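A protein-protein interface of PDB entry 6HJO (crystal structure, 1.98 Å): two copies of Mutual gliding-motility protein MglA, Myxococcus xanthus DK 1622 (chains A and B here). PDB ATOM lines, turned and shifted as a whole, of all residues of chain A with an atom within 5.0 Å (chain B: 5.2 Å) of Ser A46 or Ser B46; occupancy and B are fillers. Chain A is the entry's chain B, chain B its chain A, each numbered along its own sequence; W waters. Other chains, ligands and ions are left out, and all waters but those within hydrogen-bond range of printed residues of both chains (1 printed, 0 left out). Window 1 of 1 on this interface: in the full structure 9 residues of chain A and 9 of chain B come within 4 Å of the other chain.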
ATOM      1  N   LEU A  44      -8.050   5.012  -1.583  1.00  0.00           N
ATOM      2  CA  LEU A  44      -8.166   3.916  -2.553  1.00  0.00           C
ATOM      3  C   LEU A  44      -7.157   4.265  -3.634  1.00  0.00           C
ATOM      4  O   LEU A  44      -7.329   5.270  -4.339  1.00  0.00           O
ATOM      5  CB  LEU A  44      -9.585   3.819  -3.149  1.00  0.00           C
ATOM      6  CG  LEU A  44      -9.838   2.652  -4.137  1.00  0.00           C
ATOM      7  CD1 LEU A  44      -9.468   1.269  -3.517  1.00  0.00           C
ATOM      8  CD2 LEU A  44     -11.270   2.663  -4.630  1.00  0.00           C
ATOM      9  N   ILE A  45      -6.056   3.499  -3.699  1.00  0.00           N
ATOM     10  CA  ILE A  45      -4.961   3.817  -4.609  1.00  0.00           C
ATOM     11  C   ILE A  45      -4.929   2.911  -5.811  1.00  0.00           C
ATOM     12  O   ILE A  45      -4.874   1.697  -5.673  1.00  0.00           O
ATOM     13  CB  ILE A  45      -3.582   3.876  -3.886  1.00  0.00           C
ATOM     14  CG1 ILE A  45      -3.605   4.927  -2.744  1.00  0.00           C
ATOM     15  CG2 ILE A  45      -2.456   4.179  -4.890  1.00  0.00           C
ATOM     16  CD1 ILE A  45      -2.402   4.939  -1.791  1.00  0.00           C
ATOM     17  N   SER A  46      -4.905   3.533  -6.988  1.00  0.00           N
ATOM     18  CA  SER A  46      -4.771   2.883  -8.280  1.00  0.00           C
ATOM     19  C   SER A  46      -3.360   3.225  -8.763  1.00  0.00           C
ATOM     20  O   SER A  46      -2.973   4.394  -8.802  1.00  0.00           O
ATOM     21  CB  SER A  46      -5.820   3.409  -9.255  1.00  0.00           C
ATOM     22  OG  SER A  46      -5.717   2.767 -10.511  1.00  0.00           O
ATOM     23  N   LEU A  47      -2.582   2.199  -9.055  1.00  0.00           N
ATOM     24  CA  LEU A  47      -1.200   2.329  -9.479  1.00  0.00           C
ATOM     25  C   LEU A  47      -1.091   1.753 -10.887  1.00  0.00           C
ATOM     26  O   LEU A  47      -1.594   0.660 -11.139  1.00  0.00           O
ATOM     27  CB  LEU A  47      -0.338   1.537  -8.478  1.00  0.00           C
ATOM     28  CG  LEU A  47       1.161   1.478  -8.666  1.00  0.00           C
ATOM     29  CD1 LEU A  47       1.846   1.452  -7.310  1.00  0.00           C
ATOM     30  CD2 LEU A  47       1.578   0.260  -9.501  1.00  0.00           C
ATOM     31  N   SER A  48      -0.447   2.478 -11.798  1.00  0.00           N
ATOM     32  CA  SER A  48      -0.252   1.995 -13.147  1.00  0.00           C
ATOM     33  C   SER A  48       1.111   2.359 -13.726  1.00  0.00           C
ATOM     34  O   SER A  48       1.645   3.444 -13.473  1.00  0.00           O
ATOM     35  CB  SER A  48      -1.387   2.433 -14.071  1.00  0.00           C
ATOM     36  OG  SER A  48      -1.238   3.753 -14.564  1.00  0.00           O
ATOM     37  N   THR A  54      -2.111  -2.023 -10.320  1.00  0.00           N
ATOM     38  CA  THR A  54      -2.399  -2.427  -8.941  1.00  0.00           C
ATOM     39  C   THR A  54      -3.511  -1.541  -8.378  1.00  0.00           C
ATOM     40  O   THR A  54      -3.594  -0.357  -8.711  1.00  0.00           O
ATOM     41  CB  THR A  54      -1.116  -2.337  -8.048  1.00  0.00           C
ATOM     42  OG1 THR A  54      -0.053  -3.070  -8.651  1.00  0.00           O
ATOM     43  CG2 THR A  54      -1.327  -2.901  -6.651  1.00  0.00           C
ATOM     44  N   LEU A  55      -4.364  -2.121  -7.530  1.00  0.00           N
ATOM     45  CA  LEU A  55      -5.422  -1.409  -6.830  1.00  0.00           C
ATOM     46  C   LEU A  55      -5.337  -1.859  -5.387  1.00  0.00           C
ATOM     47  O   LEU A  55      -5.289  -3.064  -5.118  1.00  0.00           O
ATOM     48  CB  LEU A  55      -6.817  -1.695  -7.408  1.00  0.00           C
ATOM     49  CG  LEU A  55      -8.011  -0.934  -6.772  1.00  0.00           C
ATOM     50  CD1 LEU A  55      -7.948   0.589  -7.051  1.00  0.00           C
ATOM     51  CD2 LEU A  55      -9.325  -1.470  -7.283  1.00  0.00           C
ATOM     52  N   LEU B  44       8.084   4.096 -14.502  1.00  0.00           N
ATOM     53  CA  LEU B  44       7.397   5.395 -14.490  1.00  0.00           C
ATOM     54  C   LEU B  44       6.020   5.071 -13.888  1.00  0.00           C
ATOM     55  O   LEU B  44       5.235   4.342 -14.496  1.00  0.00           O
ATOM     56  CB  LEU B  44       7.264   5.994 -15.897  1.00  0.00           C
ATOM     57  CG  LEU B  44       6.607   7.400 -15.983  1.00  0.00           C
ATOM     58  CD1 LEU B  44       7.321   8.433 -15.091  1.00  0.00           C
ATOM     59  CD2 LEU B  44       6.565   7.913 -17.436  1.00  0.00           C
ATOM     60  N   ILE B  45       5.778   5.538 -12.655  1.00  0.00           N
ATOM     61  CA  ILE B  45       4.563   5.195 -11.918  1.00  0.00           C
ATOM     62  C   ILE B  45       3.575   6.327 -11.877  1.00  0.00           C
ATOM     63  O   ILE B  45       3.908   7.432 -11.451  1.00  0.00           O
ATOM     64  CB  ILE B  45       4.860   4.638 -10.497  1.00  0.00           C
ATOM     65  CG1 ILE B  45       5.778   3.382 -10.576  1.00  0.00           C
ATOM     66  CG2 ILE B  45       3.534   4.316  -9.754  1.00  0.00           C
ATOM     67  CD1 ILE B  45       6.350   2.868  -9.256  1.00  0.00           C
ATOM     68  N   SER B  46       2.336   6.007 -12.266  1.00  0.00           N
ATOM     69  CA  SER B  46       1.190   6.897 -12.231  1.00  0.00           C
ATOM     70  C   SER B  46       0.293   6.373 -11.104  1.00  0.00           C
ATOM     71  O   SER B  46      -0.038   5.185 -11.040  1.00  0.00           O
ATOM     72  CB  SER B  46       0.464   6.871 -13.572  1.00  0.00           C
ATOM     73  OG  SER B  46      -0.673   7.712 -13.571  1.00  0.00           O
ATOM     74  N   LEU B  47      -0.030   7.248 -10.179  1.00  0.00           N
ATOM     75  CA  LEU B  47      -0.843   6.925  -9.022  1.00  0.00           C
ATOM     76  C   LEU B  47      -2.105   7.788  -9.069  1.00  0.00           C
ATOM     77  O   LEU B  47      -2.019   8.998  -9.305  1.00  0.00           O
ATOM     78  CB  LEU B  47       0.005   7.230  -7.771  1.00  0.00           C
ATOM     79  CG  LEU B  47      -0.563   6.994  -6.394  1.00  0.00           C
ATOM     80  CD1 LEU B  47       0.538   6.563  -5.443  1.00  0.00           C
ATOM     81  CD2 LEU B  47      -1.250   8.252  -5.846  1.00  0.00           C
ATOM     82  N   SER B  48      -3.277   7.171  -8.860  1.00  0.00           N
ATOM     83  CA  SER B  48      -4.517   7.935  -8.823  1.00  0.00           C
ATOM     84  C   SER B  48      -5.495   7.442  -7.769  1.00  0.00           C
ATOM     85  O   SER B  48      -5.589   6.242  -7.497  1.00  0.00           O
ATOM     86  CB  SER B  48      -5.164   8.027 -10.206  1.00  0.00           C
ATOM     87  OG  SER B  48      -5.945   6.896 -10.537  1.00  0.00           O
ATOM     88  N   THR B  49      -6.185   8.404  -7.144  1.00  0.00           N
ATOM     89  CA  THR B  49      -7.257   8.242  -6.151  1.00  0.00           C
ATOM     90  C   THR B  49      -8.419   9.130  -6.658  1.00  0.00           C
ATOM     91  O   THR B  49      -8.237   9.870  -7.637  1.00  0.00           O
ATOM     92  CB  THR B  49      -6.792   8.729  -4.758  1.00  0.00           C
ATOM     93  OG1 THR B  49      -6.409  10.097  -4.853  1.00  0.00           O
ATOM     94  CG2 THR B  49      -5.640   7.930  -4.178  1.00  0.00           C
ATOM     95  N   THR B  54      -0.607  11.426  -8.816  1.00  0.00           N
ATOM     96  CA  THR B  54       0.852  11.525  -8.659  1.00  0.00           C
ATOM     97  C   THR B  54       1.533  10.817  -9.832  1.00  0.00           C
ATOM     98  O   THR B  54       1.032   9.810 -10.331  1.00  0.00           O
ATOM     99  CB  THR B  54       1.322  10.926  -7.290  1.00  0.00           C
ATOM    100  OG1 THR B  54       0.583  11.510  -6.219  1.00  0.00           O
ATOM    101  CG2 THR B  54       2.791  11.169  -7.014  1.00  0.00           C
ATOM    102  N   LEU B  55       2.675  11.358 -10.268  1.00  0.00           N
ATOM    103  CA  LEU B  55       3.517  10.769 -11.302  1.00  0.00           C
ATOM    104  C   LEU B  55       4.924  10.818 -10.772  1.00  0.00           C
ATOM    105  O   LEU B  55       5.370  11.868 -10.298  1.00  0.00           O
ATOM    106  CB  LEU B  55       3.415  11.522 -12.628  1.00  0.00           C
ATOM    107  CG  LEU B  55       4.208  10.929 -13.829  1.00  0.00           C
ATOM    108  CD1 LEU B  55       3.645   9.537 -14.282  1.00  0.00           C
ATOM    109  CD2 LEU B  55       4.240  11.938 -14.999  1.00  0.00           C
ATOM    110  N   PHE B  56       5.620   9.676 -10.807  1.00  0.00           N
ATOM    111  CA  PHE B  56       6.978   9.614 -10.269  1.00  0.00           C
ATOM    112  C   PHE B  56       7.797   8.468 -10.818  1.00  0.00           C
ATOM    113  O   PHE B  56       7.242   7.477 -11.308  1.00  0.00           O
ATOM    114  CB  PHE B  56       6.956   9.562  -8.723  1.00  0.00           C
ATOM    115  CG  PHE B  56       6.348   8.320  -8.115  1.00  0.00           C
ATOM    116  CD1 PHE B  56       4.977   8.235  -7.891  1.00  0.00           C
ATOM    117  CD2 PHE B  56       7.147   7.246  -7.749  1.00  0.00           C
ATOM    118  CE1 PHE B  56       4.414   7.087  -7.327  1.00  0.00           C
ATOM    119  CE2 PHE B  56       6.584   6.090  -7.172  1.00  0.00           C
ATOM    120  CZ  PHE B  56       5.221   6.020  -6.968  1.00  0.00           C
HETATM  121  O   HOH W   1      -2.768   4.979 -11.906  1.00  0.00           O
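The backbone NH (N) of Ser A48 lies within hydrogen-bond range of the backbone carbonyl oxygen (O) of Ser B46, at 2.8 Å.
The backbone carbonyl oxygen (O) of Ser A46 is in hydrogen-bond range of the backbone NH (N) of Ser B48.
O of Phe B56 sits at hydrogen-bond distance from N of Ile B45 (2.8 Å).
The backbone carbonyl oxygen (O) of Thr B54 sits at hydrogen-bond distance from the backbone NH (N) of Leu B47, at 2.8 Å.
O of Thr A54 lies within hydrogen-bond range of N of Leu A47 (2.8 Å).
Among the printed residues, pairs that only touch across the chains: Leu A44 with Thr B49 (3.2 Å), Ser A46 with Leu B47 (3.3 Å), Leu A47 with Ser B46 (3.5 Å), Ile A45 with Leu B47 (3.7 Å), Leu A44 with Ser B48 (3.7 Å), Ser A48 with Ile B45 (3.7 Å), Ser A46 with Ser B46 (3.8 Å), Ile A45 with Ser B48 (3.8 Å), Ser A48 with Leu B44 (3.8 Å), Leu A47 with Ile B45 (3.9 Å) and Ile A45 with Thr B49 (3.9 Å).
Ser B46 touches just these residues of chain A: Ser A46, Leu A47 and Ser A48.
Printed residues of chain B within 4 Å of Leu A44: Ser B48 and Thr B49.
Printed residues of chain A within 4 Å of Leu B47: Ile A45 and Ser A46.
Of the printed residues of chain A, Leu B44 touches Ser A48.
Printed residues of chain B within 4 Å of Ser A48: Leu B44 (3.8 Å), Ile B45 (3.7 Å) and Ser B46 (2.8 Å).
Of the printed residues of chain A, Thr B49 touches Leu A44 (3.2 Å) and Ile A45 (3.9 Å).
Leu A55 touches none of the printed residues of chain B.
Leu B55 touches none of the printed residues of chain A.
The nearest residue of chain B that does not touch Ser A46 is Thr B49 (5.0 Å).
The nearest printed residue of chain A that does not touch Ser B46 is Ile A45 (6.7 Å).
The nearest printed residue of chain A that does not touch Leu B47 is Leu A47 (4.6 Å).
Along chain B the printed residues that touch a printed residue of chain A span positions 44 to 49.
Of the 7 printed residues of chain A, 5 touch a printed residue of chain B.
Hydrophobic or aromatic side chains of chain A that line the printed part of chain B: Ile A45 and Leu A47.
Along chain A the printed residues that touch a printed residue of chain B span positions 44 to 48.
Ile A45 touches Leu B47, and with the chains exchanged Leu A47 touches Ile B45.
Ile A45 touches Ser B48, and with the chains exchanged Ser A48 touches Ile B45.
Ser B46 touches its own counterpart, Ser A46.
Ser A46 touches Ser B48, and with the chains exchanged Ser A48 touches Ser B46.
Of the 13 pairs that touch across the chains among the printed residues, 11 have their exchanged pair printed and touching as well.
Water W1 lies within hydrogen-bond range of the backbone carbonyl oxygen of Ser B46 (2.9 Å), the backbone carbonyl oxygen of Ser A46 (3.2 Å) and the side-chain hydroxyl of Ser A48 (3.3 Å).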
